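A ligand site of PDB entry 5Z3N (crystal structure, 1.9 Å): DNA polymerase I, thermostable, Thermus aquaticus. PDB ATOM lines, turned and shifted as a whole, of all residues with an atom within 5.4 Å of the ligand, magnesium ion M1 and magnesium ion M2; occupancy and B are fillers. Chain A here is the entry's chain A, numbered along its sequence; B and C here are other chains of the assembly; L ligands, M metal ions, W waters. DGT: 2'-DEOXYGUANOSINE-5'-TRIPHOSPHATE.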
ATOM      1  N   ARG A 280     -26.664   1.963 -27.018  1.00  0.00           N
ATOM      2  CA  ARG A 280     -26.109   3.285 -27.247  1.00  0.00           C
ATOM      3  C   ARG A 280     -26.459   3.799 -28.636  1.00  0.00           C
ATOM      4  O   ARG A 280     -26.714   3.035 -29.560  1.00  0.00           O
ATOM      5  CB  ARG A 280     -24.611   3.221 -27.150  1.00  0.00           C
ATOM      6  CG  ARG A 280     -24.108   3.249 -25.738  1.00  0.00           C
ATOM      7  CD  ARG A 280     -22.608   3.402 -25.835  1.00  0.00           C
ATOM      8  NE  ARG A 280     -22.024   3.705 -24.558  1.00  0.00           N
ATOM      9  CZ  ARG A 280     -20.747   3.980 -24.384  1.00  0.00           C
ATOM     10  NH1 ARG A 280     -19.901   3.948 -25.418  1.00  0.00           N
ATOM     11  NH2 ARG A 280     -20.313   4.284 -23.161  1.00  0.00           N
ATOM     12  N   ASP A 317     -22.570  16.132 -18.148  1.00  0.00           N
ATOM     13  CA  ASP A 317     -21.957  14.804 -18.187  1.00  0.00           C
ATOM     14  C   ASP A 317     -22.269  14.072 -16.896  1.00  0.00           C
ATOM     15  O   ASP A 317     -21.960  14.576 -15.820  1.00  0.00           O
ATOM     16  CB  ASP A 317     -20.426  14.950 -18.336  1.00  0.00           C
ATOM     17  CG  ASP A 317     -19.748  13.642 -18.624  1.00  0.00           C
ATOM     18  OD1 ASP A 317     -19.958  12.665 -17.877  1.00  0.00           O
ATOM     19  OD2 ASP A 317     -18.957  13.590 -19.603  1.00  0.00           O
ATOM     20  N   TYR A 318     -22.884  12.897 -16.999  1.00  0.00           N
ATOM     21  CA  TYR A 318     -23.183  12.100 -15.813  1.00  0.00           C
ATOM     22  C   TYR A 318     -21.901  11.657 -15.119  1.00  0.00           C
ATOM     23  O   TYR A 318     -20.944  11.226 -15.770  1.00  0.00           O
ATOM     24  CB  TYR A 318     -23.982  10.863 -16.163  1.00  0.00           C
ATOM     25  CG  TYR A 318     -25.454  11.058 -16.403  1.00  0.00           C
ATOM     26  CD1 TYR A 318     -26.330  11.237 -15.330  1.00  0.00           C
ATOM     27  CD2 TYR A 318     -26.000  10.975 -17.681  1.00  0.00           C
ATOM     28  CE1 TYR A 318     -27.708  11.377 -15.525  1.00  0.00           C
ATOM     29  CE2 TYR A 318     -27.366  11.105 -17.895  1.00  0.00           C
ATOM     30  CZ  TYR A 318     -28.211  11.321 -16.796  1.00  0.00           C
ATOM     31  OH  TYR A 318     -29.552  11.435 -16.982  1.00  0.00           O
ATOM     32  N   SER A 319     -21.880  11.795 -13.812  1.00  0.00           N
ATOM     33  CA  SER A 319     -20.760  11.403 -12.960  1.00  0.00           C
ATOM     34  C   SER A 319     -20.691   9.880 -12.774  1.00  0.00           C
ATOM     35  O   SER A 319     -21.616   9.279 -12.275  1.00  0.00           O
ATOM     36  CB  SER A 319     -20.916  12.067 -11.592  1.00  0.00           C
ATOM     37  OG  SER A 319     -20.069  11.508 -10.622  1.00  0.00           O
ATOM     38  N   GLN A 320     -19.567   9.248 -13.133  1.00  0.00           N
ATOM     39  CA  GLN A 320     -19.309   7.849 -12.804  1.00  0.00           C
ATOM     40  C   GLN A 320     -20.469   6.925 -13.153  1.00  0.00           C
ATOM     41  O   GLN A 320     -20.827   6.021 -12.371  1.00  0.00           O
ATOM     42  CB  GLN A 320     -19.017   7.703 -11.321  1.00  0.00           C
ATOM     43  CG  GLN A 320     -17.884   8.585 -10.830  1.00  0.00           C
ATOM     44  CD  GLN A 320     -17.724   8.507  -9.338  1.00  0.00           C
ATOM     45  OE1 GLN A 320     -17.124   7.575  -8.829  1.00  0.00           O
ATOM     46  NE2 GLN A 320     -18.280   9.474  -8.634  1.00  0.00           N
ATOM     47  N   ILE A 321     -21.020   7.138 -14.319  1.00  0.00           N
ATOM     48  CA  ILE A 321     -22.355   6.647 -14.591  1.00  0.00           C
ATOM     49  C   ILE A 321     -22.512   5.126 -14.550  1.00  0.00           C
ATOM     50  O   ILE A 321     -23.400   4.645 -13.845  1.00  0.00           O
ATOM     51  CB  ILE A 321     -22.964   7.270 -15.882  1.00  0.00           C
ATOM     52  CG1 ILE A 321     -24.442   6.900 -16.007  1.00  0.00           C
ATOM     53  CG2 ILE A 321     -22.294   6.819 -17.150  1.00  0.00           C
ATOM     54  CD1 ILE A 321     -25.301   7.384 -14.860  1.00  0.00           C
ATOM     55  N   GLU A 322     -21.664   4.359 -15.252  1.00  0.00           N
ATOM     56  CA  GLU A 322     -21.810   2.898 -15.220  1.00  0.00           C
ATOM     57  C   GLU A 322     -21.564   2.296 -13.811  1.00  0.00           C
ATOM     58  O   GLU A 322     -22.149   1.286 -13.500  1.00  0.00           O
ATOM     59  CB  GLU A 322     -20.999   2.211 -16.324  1.00  0.00           C
ATOM     60  CG  GLU A 322     -21.662   2.416 -17.686  1.00  0.00           C
ATOM     61  CD  GLU A 322     -20.957   1.767 -18.859  1.00  0.00           C
ATOM     62  OE1 GLU A 322     -20.267   0.747 -18.679  1.00  0.00           O
ATOM     63  OE2 GLU A 322     -21.091   2.301 -19.964  1.00  0.00           O
ATOM     64  N   LEU A 323     -20.784   2.968 -12.969  1.00  0.00           N
ATOM     65  CA  LEU A 323     -20.577   2.505 -11.595  1.00  0.00           C
ATOM     66  C   LEU A 323     -21.826   2.694 -10.728  1.00  0.00           C
ATOM     67  O   LEU A 323     -22.116   1.848  -9.878  1.00  0.00           O
ATOM     68  CB  LEU A 323     -19.344   3.151 -10.932  1.00  0.00           C
ATOM     69  CG  LEU A 323     -17.986   2.864 -11.605  1.00  0.00           C
ATOM     70  CD1 LEU A 323     -16.847   3.557 -10.856  1.00  0.00           C
ATOM     71  CD2 LEU A 323     -17.709   1.362 -11.678  1.00  0.00           C
ATOM     72  N   ASP A 344     -15.941   9.742  -5.004  1.00  0.00           N
ATOM     73  CA  ASP A 344     -15.525   9.567  -6.386  1.00  0.00           C
ATOM     74  C   ASP A 344     -14.484   8.448  -6.503  1.00  0.00           C
ATOM     75  O   ASP A 344     -13.357   8.587  -6.047  1.00  0.00           O
ATOM     76  CB  ASP A 344     -14.973  10.863  -6.966  1.00  0.00           C
ATOM     77  CG  ASP A 344     -14.882  10.843  -8.456  1.00  0.00           C
ATOM     78  OD1 ASP A 344     -14.356   9.849  -9.022  1.00  0.00           O
ATOM     79  OD2 ASP A 344     -15.305  11.819  -9.096  1.00  0.00           O
ATOM     80  N   HIS A 346     -13.174   7.161  -9.358  1.00  0.00           N
ATOM     81  CA  HIS A 346     -12.110   7.466 -10.324  1.00  0.00           C
ATOM     82  C   HIS A 346     -10.993   8.264  -9.665  1.00  0.00           C
ATOM     83  O   HIS A 346      -9.815   7.946  -9.844  1.00  0.00           O
ATOM     84  CB  HIS A 346     -12.646   8.231 -11.551  1.00  0.00           C
ATOM     85  CG  HIS A 346     -13.693   7.488 -12.312  1.00  0.00           C
ATOM     86  ND1 HIS A 346     -13.678   6.109 -12.473  1.00  0.00           N
ATOM     87  CD2 HIS A 346     -14.790   7.917 -12.975  1.00  0.00           C
ATOM     88  CE1 HIS A 346     -14.727   5.731 -13.174  1.00  0.00           C
ATOM     89  NE2 HIS A 346     -15.416   6.809 -13.494  1.00  0.00           N
ATOM     90  N   ARG A 366      -7.186  10.987 -14.125  1.00  0.00           N
ATOM     91  CA  ARG A 366      -8.550  10.519 -13.975  1.00  0.00           C
ATOM     92  C   ARG A 366      -8.921   9.596 -15.143  1.00  0.00           C
ATOM     93  O   ARG A 366      -9.519   8.574 -14.913  1.00  0.00           O
ATOM     94  CB  ARG A 366      -9.561  11.698 -13.858  1.00  0.00           C
ATOM     95  CG  ARG A 366     -10.983  11.249 -13.569  1.00  0.00           C
ATOM     96  CD  ARG A 366     -12.064  12.331 -13.836  1.00  0.00           C
ATOM     97  NE  ARG A 366     -13.422  11.856 -13.505  1.00  0.00           N
ATOM     98  CZ  ARG A 366     -13.842  11.648 -12.267  1.00  0.00           C
ATOM     99  NH1 ARG A 366     -15.068  11.220 -12.044  1.00  0.00           N
ATOM    100  NH2 ARG A 366     -13.042  11.853 -11.226  1.00  0.00           N
ATOM    101  N   ARG A 367      -8.517   9.947 -16.368  1.00  0.00           N
ATOM    102  CA  ARG A 367      -8.765   9.062 -17.534  1.00  0.00           C
ATOM    103  C   ARG A 367      -8.016   7.728 -17.392  1.00  0.00           C
ATOM    104  O   ARG A 367      -8.550   6.655 -17.684  1.00  0.00           O
ATOM    105  CB  ARG A 367      -8.425   9.788 -18.846  1.00  0.00           C
ATOM    106  CG  ARG A 367      -8.672   9.011 -20.164  1.00  0.00           C
ATOM    107  CD  ARG A 367     -10.096   8.424 -20.355  1.00  0.00           C
ATOM    108  NE  ARG A 367     -10.146   7.015 -19.982  1.00  0.00           N
ATOM    109  CZ  ARG A 367     -11.150   6.169 -20.194  1.00  0.00           C
ATOM    110  NH1 ARG A 367     -10.983   4.886 -19.830  1.00  0.00           N
ATOM    111  NH2 ARG A 367     -12.296   6.542 -20.773  1.00  0.00           N
ATOM    112  N   LYS A 370      -9.966   5.651 -14.986  1.00  0.00           N
ATOM    113  CA  LYS A 370     -11.165   5.089 -15.621  1.00  0.00           C
ATOM    114  C   LYS A 370     -10.884   3.747 -16.298  1.00  0.00           C
ATOM    115  O   LYS A 370     -11.675   2.781 -16.183  1.00  0.00           O
ATOM    116  CB  LYS A 370     -11.756   6.074 -16.641  1.00  0.00           C
ATOM    117  CG  LYS A 370     -12.569   7.176 -16.009  1.00  0.00           C
ATOM    118  CD  LYS A 370     -13.144   8.117 -17.064  1.00  0.00           C
ATOM    119  CE  LYS A 370     -13.778   9.331 -16.429  1.00  0.00           C
ATOM    120  NZ  LYS A 370     -14.138  10.348 -17.453  1.00  0.00           N
ATOM    121  N   THR A 371      -9.757   3.677 -16.992  1.00  0.00           N
ATOM    122  CA  THR A 371      -9.329   2.447 -17.639  1.00  0.00           C
ATOM    123  C   THR A 371      -9.203   1.314 -16.639  1.00  0.00           C
ATOM    124  O   THR A 371      -9.665   0.199 -16.901  1.00  0.00           O
ATOM    125  CB  THR A 371      -8.028   2.667 -18.415  1.00  0.00           C
ATOM    126  OG1 THR A 371      -8.270   3.666 -19.418  1.00  0.00           O
ATOM    127  CG2 THR A 371      -7.559   1.398 -19.078  1.00  0.00           C
ATOM    128  N   PHE A 374     -13.017   0.487 -14.967  1.00  0.00           N
ATOM    129  CA  PHE A 374     -13.888  -0.249 -15.882  1.00  0.00           C
ATOM    130  C   PHE A 374     -13.220  -1.525 -16.389  1.00  0.00           C
ATOM    131  O   PHE A 374     -13.874  -2.553 -16.474  1.00  0.00           O
ATOM    132  CB  PHE A 374     -14.379   0.644 -17.014  1.00  0.00           C
ATOM    133  CG  PHE A 374     -15.203   1.805 -16.513  1.00  0.00           C
ATOM    134  CD1 PHE A 374     -16.339   1.583 -15.752  1.00  0.00           C
ATOM    135  CD2 PHE A 374     -14.836   3.124 -16.776  1.00  0.00           C
ATOM    136  CE1 PHE A 374     -17.107   2.640 -15.262  1.00  0.00           C
ATOM    137  CE2 PHE A 374     -15.600   4.188 -16.293  1.00  0.00           C
ATOM    138  CZ  PHE A 374     -16.738   3.939 -15.545  1.00  0.00           C
ATOM    139  N   GLY A 375     -11.921  -1.440 -16.689  1.00  0.00           N
ATOM    140  CA  GLY A 375     -11.101  -2.607 -16.999  1.00  0.00           C
ATOM    141  C   GLY A 375     -11.282  -3.727 -16.009  1.00  0.00           C
ATOM    142  O   GLY A 375     -11.717  -4.814 -16.380  1.00  0.00           O
ATOM    143  N   TYR A 378     -15.008  -5.109 -15.927  1.00  0.00           N
ATOM    144  CA  TYR A 378     -15.434  -5.859 -17.105  1.00  0.00           C
ATOM    145  C   TYR A 378     -14.466  -6.986 -17.535  1.00  0.00           C
ATOM    146  O   TYR A 378     -14.596  -7.515 -18.640  1.00  0.00           O
ATOM    147  CB  TYR A 378     -15.727  -4.900 -18.256  1.00  0.00           C
ATOM    148  CG  TYR A 378     -16.878  -3.963 -17.941  1.00  0.00           C
ATOM    149  CD1 TYR A 378     -18.123  -4.462 -17.554  1.00  0.00           C
ATOM    150  CD2 TYR A 378     -16.720  -2.589 -18.024  1.00  0.00           C
ATOM    151  CE1 TYR A 378     -19.184  -3.631 -17.264  1.00  0.00           C
ATOM    152  CE2 TYR A 378     -17.766  -1.731 -17.760  1.00  0.00           C
ATOM    153  CZ  TYR A 378     -19.004  -2.257 -17.365  1.00  0.00           C
ATOM    154  OH  TYR A 378     -20.061  -1.399 -17.092  1.00  0.00           O
ATOM    155  N   ASN A 457     -21.433  -6.892 -19.634  1.00  0.00           N
ATOM    156  CA  ASN A 457     -21.255  -5.470 -19.857  1.00  0.00           C
ATOM    157  C   ASN A 457     -22.537  -4.803 -20.323  1.00  0.00           C
ATOM    158  O   ASN A 457     -22.812  -3.646 -19.954  1.00  0.00           O
ATOM    159  CB  ASN A 457     -20.144  -5.219 -20.865  1.00  0.00           C
ATOM    160  CG  ASN A 457     -20.069  -3.771 -21.306  1.00  0.00           C
ATOM    161  OD1 ASN A 457     -20.705  -3.370 -22.267  1.00  0.00           O
ATOM    162  ND2 ASN A 457     -19.339  -2.976 -20.567  1.00  0.00           N
ATOM    163  N   VAL A 490     -23.125  12.436 -26.362  1.00  0.00           N
ATOM    164  CA  VAL A 490     -21.839  11.713 -26.336  1.00  0.00           C
ATOM    165  C   VAL A 490     -21.919  10.694 -25.186  1.00  0.00           C
ATOM    166  O   VAL A 490     -21.104  10.693 -24.267  1.00  0.00           O
ATOM    167  CB  VAL A 490     -20.560  12.614 -26.218  1.00  0.00           C
ATOM    168  CG1 VAL A 490     -19.280  11.828 -26.535  1.00  0.00           C
ATOM    169  CG2 VAL A 490     -20.650  13.815 -27.143  1.00  0.00           C
ATOM    170  N   ASP A 492     -22.991   9.669 -22.324  1.00  0.00           N
ATOM    171  CA  ASP A 492     -23.532  10.101 -21.045  1.00  0.00           C
ATOM    172  C   ASP A 492     -23.450  11.615 -20.891  1.00  0.00           C
ATOM    173  O   ASP A 492     -23.501  12.133 -19.780  1.00  0.00           O
ATOM    174  CB  ASP A 492     -22.808   9.424 -19.882  1.00  0.00           C
ATOM    175  CG  ASP A 492     -21.450  10.002 -19.616  1.00  0.00           C
ATOM    176  OD1 ASP A 492     -20.787  10.469 -20.571  1.00  0.00           O
ATOM    177  OD2 ASP A 492     -21.036  10.031 -18.437  1.00  0.00           O
ATOM    178  N   GLU A 493     -23.347  12.304 -22.024  1.00  0.00           N
ATOM    179  CA  GLU A 493     -23.159  13.736 -22.062  1.00  0.00           C
ATOM    180  C   GLU A 493     -24.079  14.320 -23.095  1.00  0.00           C
ATOM    181  O   GLU A 493     -24.268  13.748 -24.170  1.00  0.00           O
ATOM    182  CB  GLU A 493     -21.687  14.071 -22.422  1.00  0.00           C
ATOM    183  CG  GLU A 493     -21.394  15.536 -22.749  1.00  0.00           C
ATOM    184  CD  GLU A 493     -19.972  15.798 -23.242  1.00  0.00           C
ATOM    185  OE1 GLU A 493     -19.190  14.847 -23.401  1.00  0.00           O
ATOM    186  OE2 GLU A 493     -19.653  16.992 -23.430  1.00  0.00           O
ATOM    187  N   LYS A 538     -16.719  22.187 -20.238  1.00  0.00           N
ATOM    188  CA  LYS A 538     -16.558  21.053 -19.296  1.00  0.00           C
ATOM    189  C   LYS A 538     -15.545  21.324 -18.202  1.00  0.00           C
ATOM    190  O   LYS A 538     -15.216  20.413 -17.444  1.00  0.00           O
ATOM    191  CB  LYS A 538     -16.129  19.808 -20.049  1.00  0.00           C
ATOM    192  CG  LYS A 538     -17.148  19.371 -21.084  1.00  0.00           C
ATOM    193  CD  LYS A 538     -17.012  17.906 -21.462  1.00  0.00           C
ATOM    194  CE  LYS A 538     -17.574  16.968 -20.417  1.00  0.00           C
ATOM    195  NZ  LYS A 538     -17.469  15.550 -20.919  1.00  0.00           N
ATOM    196  P    DC B   4      -7.595  -8.085 -21.205  1.00  0.00           P
ATOM    197  OP1  DC B   4      -7.080  -7.255 -22.325  1.00  0.00           O
ATOM    198  OP2  DC B   4      -6.723  -8.432 -20.065  1.00  0.00           O
ATOM    199  O5'  DC B   4      -8.884  -7.280 -20.735  1.00  0.00           O
ATOM    200  C5'  DC B   4      -9.855  -6.839 -21.696  1.00  0.00           C
ATOM    201  C4'  DC B   4     -11.170  -6.584 -21.015  1.00  0.00           C
ATOM    202  O4'  DC B   4     -11.015  -5.549 -20.013  1.00  0.00           O
ATOM    203  C3'  DC B   4     -12.289  -6.109 -21.921  1.00  0.00           C
ATOM    204  O3'  DC B   4     -12.926  -7.222 -22.528  1.00  0.00           O
ATOM    205  C2'  DC B   4     -13.174  -5.332 -20.968  1.00  0.00           C
ATOM    206  C1'  DC B   4     -12.146  -4.680 -20.033  1.00  0.00           C
ATOM    207  N1   DC B   4     -11.691  -3.329 -20.443  1.00  0.00           N
ATOM    208  C2   DC B   4     -12.598  -2.262 -20.332  1.00  0.00           C
ATOM    209  O2   DC B   4     -13.741  -2.487 -19.915  1.00  0.00           O
ATOM    210  N3   DC B   4     -12.202  -1.024 -20.692  1.00  0.00           N
ATOM    211  C4   DC B   4     -10.959  -0.826 -21.155  1.00  0.00           C
ATOM    212  N4   DC B   4     -10.617   0.415 -21.512  1.00  0.00           N
ATOM    213  C5   DC B   4     -10.032  -1.900 -21.307  1.00  0.00           C
ATOM    214  C6   DC B   4     -10.440  -3.118 -20.919  1.00  0.00           C
ATOM    215  P    DG B   5     -13.359  -7.181 -24.077  1.00  0.00           P
ATOM    216  OP1  DG B   5     -13.773  -8.545 -24.455  1.00  0.00           O
ATOM    217  OP2  DG B   5     -12.329  -6.470 -24.834  1.00  0.00           O
ATOM    218  O5'  DG B   5     -14.674  -6.294 -24.061  1.00  0.00           O
ATOM    219  C5'  DG B   5     -15.880  -6.773 -23.478  1.00  0.00           C
ATOM    220  C4'  DG B   5     -16.911  -5.669 -23.448  1.00  0.00           C
ATOM    221  O4'  DG B   5     -16.385  -4.578 -22.665  1.00  0.00           O
ATOM    222  C3'  DG B   5     -17.242  -5.047 -24.793  1.00  0.00           C
ATOM    223  O3'  DG B   5     -18.313  -5.735 -25.420  1.00  0.00           O
ATOM    224  C2'  DG B   5     -17.699  -3.655 -24.399  1.00  0.00           C
ATOM    225  C1'  DG B   5     -16.839  -3.350 -23.190  1.00  0.00           C
ATOM    226  N9   DG B   5     -15.681  -2.507 -23.462  1.00  0.00           N
ATOM    227  C8   DG B   5     -14.356  -2.853 -23.598  1.00  0.00           C
ATOM    228  N7   DG B   5     -13.576  -1.831 -23.802  1.00  0.00           N
ATOM    229  C5   DG B   5     -14.443  -0.736 -23.808  1.00  0.00           C
ATOM    230  C6   DG B   5     -14.174   0.643 -23.989  1.00  0.00           C
ATOM    231  O6   DG B   5     -13.093   1.201 -24.166  1.00  0.00           O
ATOM    232  N1   DG B   5     -15.352   1.396 -23.955  1.00  0.00           N
ATOM    233  C2   DG B   5     -16.605   0.877 -23.762  1.00  0.00           C
ATOM    234  N2   DG B   5     -17.619   1.758 -23.734  1.00  0.00           N
ATOM    235  N3   DG B   5     -16.865  -0.403 -23.582  1.00  0.00           N
ATOM    236  C4   DG B   5     -15.737  -1.146 -23.621  1.00  0.00           C
ATOM    237  N1  DOC C  12     -16.219   6.361 -24.001  1.00  0.00           N
ATOM    238  C2  DOC C  12     -16.286   4.973 -24.018  1.00  0.00           C
ATOM    239  N3  DOC C  12     -15.172   4.265 -23.922  1.00  0.00           N
ATOM    240  C4  DOC C  12     -13.976   4.842 -23.812  1.00  0.00           C
ATOM    241  C5  DOC C  12     -13.893   6.214 -23.786  1.00  0.00           C
ATOM    242  C6  DOC C  12     -15.075   6.948 -23.865  1.00  0.00           C
ATOM    243  O2  DOC C  12     -17.363   4.421 -24.143  1.00  0.00           O
ATOM    244  N4  DOC C  12     -12.886   4.108 -23.710  1.00  0.00           N
ATOM    245  C1' DOC C  12     -17.478   7.123 -24.127  1.00  0.00           C
ATOM    246  C2' DOC C  12     -18.117   7.389 -22.766  1.00  0.00           C
ATOM    247  C3' DOC C  12     -17.700   8.795 -22.481  1.00  0.00           C
ATOM    248  C4' DOC C  12     -17.624   9.360 -23.895  1.00  0.00           C
ATOM    249  O4' DOC C  12     -17.240   8.343 -24.736  1.00  0.00           O
ATOM    250  C5' DOC C  12     -16.680  10.573 -24.038  1.00  0.00           C
ATOM    251  O5' DOC C  12     -15.344  10.295 -23.684  1.00  0.00           O
ATOM    252  P   DOC C  12     -14.287  11.402 -23.716  1.00  0.00           P
ATOM    253  OP1 DOC C  12     -14.803  12.649 -23.227  1.00  0.00           O
ATOM    254  OP2 DOC C  12     -13.123  10.876 -23.160  1.00  0.00           O
HETATM  255  PG  DGT L   1     -16.988  11.072 -15.109  1.00  0.00           P
HETATM  256  O1G DGT L   1     -18.011  11.509 -16.121  1.00  0.00           O
HETATM  257  O2G DGT L   1     -15.582  11.507 -15.405  1.00  0.00           O
HETATM  258  O3G DGT L   1     -17.387  11.228 -13.674  1.00  0.00           O
HETATM  259  O3B DGT L   1     -16.909   9.450 -15.248  1.00  0.00           O
HETATM  260  PB  DGT L   1     -17.789   8.433 -16.130  1.00  0.00           P
HETATM  261  O1B DGT L   1     -17.618   7.109 -15.467  1.00  0.00           O
HETATM  262  O2B DGT L   1     -19.210   8.866 -16.376  1.00  0.00           O
HETATM  263  O3A DGT L   1     -16.896   8.384 -17.478  1.00  0.00           O
HETATM  264  PA  DGT L   1     -17.225   9.027 -18.907  1.00  0.00           P
HETATM  265  O1A DGT L   1     -15.929   9.353 -19.548  1.00  0.00           O
HETATM  266  O2A DGT L   1     -18.181  10.181 -18.768  1.00  0.00           O
HETATM  267  O5' DGT L   1     -17.856   7.782 -19.692  1.00  0.00           O
HETATM  268  C5' DGT L   1     -19.210   7.374 -19.553  1.00  0.00           C
HETATM  269  C4' DGT L   1     -19.321   5.862 -19.414  1.00  0.00           C
HETATM  270  O4' DGT L   1     -18.874   5.190 -20.607  1.00  0.00           O
HETATM  271  C3' DGT L   1     -18.517   5.285 -18.257  1.00  0.00           C
HETATM  272  O3' DGT L   1     -19.235   5.308 -17.019  1.00  0.00           O
HETATM  273  C2' DGT L   1     -18.269   3.883 -18.721  1.00  0.00           C
HETATM  274  C1' DGT L   1     -18.173   3.999 -20.240  1.00  0.00           C
HETATM  275  N9  DGT L   1     -16.714   4.050 -20.449  1.00  0.00           N
HETATM  276  C8  DGT L   1     -15.891   5.120 -20.516  1.00  0.00           C
HETATM  277  N7  DGT L   1     -14.600   4.718 -20.638  1.00  0.00           N
HETATM  278  C5  DGT L   1     -14.603   3.384 -20.624  1.00  0.00           C
HETATM  279  C6  DGT L   1     -13.597   2.296 -20.684  1.00  0.00           C
HETATM  280  O6  DGT L   1     -12.388   2.586 -20.796  1.00  0.00           O
HETATM  281  N1  DGT L   1     -14.031   1.026 -20.641  1.00  0.00           N
HETATM  282  C2  DGT L   1     -15.336   0.699 -20.499  1.00  0.00           C
HETATM  283  N2  DGT L   1     -15.723  -0.588 -20.445  1.00  0.00           N
HETATM  284  N3  DGT L   1     -16.310   1.637 -20.435  1.00  0.00           N
HETATM  285  C4  DGT L   1     -15.986   2.946 -20.487  1.00  0.00           C
HETATM  286 MG    MG M   1     -19.564  10.666 -17.200  1.00  0.00          MG
HETATM  287 MG    MG M   2     -18.893  11.541 -20.616  1.00  0.00          MG
HETATM  288  O   HOH W   1     -16.329  12.973 -18.120  1.00  0.00           O
HETATM  289  O   HOH W   2     -13.567   8.992 -20.822  1.00  0.00           O
HETATM  290  O   HOH W   3     -19.235  13.915 -15.202  1.00  0.00           O
HETATM  291  O   HOH W   4     -17.878  13.795 -12.521  1.00  0.00           O
HETATM  292  O   HOH W   5     -22.221   4.671 -20.783  1.00  0.00           O
HETATM  293  O   HOH W   6     -19.229  12.189 -22.815  1.00  0.00           O
HETATM  294  O   HOH W   7     -19.000   0.092 -20.979  1.00  0.00           O
HETATM  295  O   HOH W   8     -16.297  11.834 -20.935  1.00  0.00           O
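N3 of DC 4 of chain B sits at hydrogen-bond distance from N1 of the ligand. O2G of the ligand lies within salt-bridge range of NZ of Lys 370, 2.8 Å away. NH1 of Arg 366 lies within salt-bridge range of O3G of the ligand (2.8 Å). An oxygen (O6) of the ligand lies within hydrogen-bond range of the guanidinium group (NH1) of Arg 367 (2.9 Å). An oxygen (O1B) of the ligand sits at hydrogen-bond distance from a ring nitrogen (NE2) of His 346. O3G of the ligand sits at hydrogen-bond distance from N of Gln 320 (3.0 Å). NH2 of Arg 280 is in hydrogen-bond range of O4' of the ligand. N of Glu 322 lies within hydrogen-bond range of O3' of the ligand (3.2 Å). N3 of DG 5 of chain B lies close to a nitrogen (N2) of the ligand. N of Ile 321 sits close to O2B of the ligand (3.2 Å).
NZ of Lys 538 sits close to OD2 of Asp 317 (2.8 Å). The guanidinium group of Arg 366 is in salt-bridge range of the side-chain carboxylate of Asp 344, 3.0 Å away. The side-chain hydroxyl (OG1) of Thr 371 sits at hydrogen-bond distance from the guanidinium group (NH1) of Arg 367 (3.0 Å). O2 of DOC 12 of chain C is in hydrogen-bond range of the guanidinium group (NH1) of Arg 280 (2.9 Å). The side-chain carboxylate (OD1) of Asp 344 is in hydrogen-bond range of the backbone NH (N) of His 346 (3.0 Å). The side-chain hydroxyl of Ser 319 sits at hydrogen-bond distance from the side-chain amide nitrogen of Gln 320, at 3.4 Å. NH2 of Arg 280 is in salt-bridge range of OE2 of Glu 322. The side-chain carboxylate of Glu 322 is in hydrogen-bond range of the side-chain hydroxyl of Tyr 378 (2.7 Å).
O6 of the ligand lies close to N4 of DOC 12 of chain C, at 3.3 Å. Merely in contact with the ligand: Ser 319, Phe 374 and Tyr 378. Hydrophobic or aromatic side chains within 4 Å of the ligand: Ile 321, His 346, Phe 374 and Tyr 378. Of the 25 residues printed, 17 come within 4 Å of the ligand. The nearest printed residue that does not touch the ligand is Asn 457 (4.3 Å).
Within 4 Å of magnesium ion M1: Asp 317, Tyr 318 and Asp 492.
Merely in contact with magnesium ion M2: DOC 12 of chain C.
Magnesium ion M1 is bound by an oxygen (O2B) of the ligand, 2.0 Å away. Magnesium ion M1 is bound by OD2 of Asp 492 (2.0 Å). O of Tyr 318 binds magnesium ion M1 (2.1 Å). Magnesium ion M1 is bound by O1G of the ligand (2.1 Å). O2A of the ligand binds magnesium ion M1, 2.1 Å away. Magnesium ion M1 is bound by OD1 of Asp 317, 2.1 Å away. Magnesium ion M1 has six donor atoms within binding distance.
Magnesium ion M2 is bound by the side-chain carboxylate (OD1) of Asp 492 (2.2 Å), the side-chain carboxylate (OD2) of Asp 317 (2.3 Å), water W6 (2.3 Å) and an oxygen (O2A) of the ligand (2.4 Å). Slightly farther from magnesium ion M2 lies water W8 (2.6 Å).
Water W6 lies within hydrogen-bond range of the side-chain carboxylate (OE1) of Glu 493 and the backbone carbonyl oxygen (O) of Val 490. Water W8 bridges OP1 of DOC 12 of chain C (2.9 Å) and O1A of the ligand (2.9 Å). Water W2 lies within hydrogen-bond range of O1A of the ligand (2.7 Å), NH2 of Arg 367 (2.8 Å) and OP2 of DOC 12 of chain C (3.0 Å). Water W1 lies within hydrogen-bond range of O2G of the ligand (3.2 Å) and NZ of Lys 370 (3.5 Å). Water W5 lies within hydrogen-bond range of OE2 of Glu 322 (2.8 Å), NH2 of Arg 280 (3.1 Å) and O4' of the ligand (3.4 Å).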
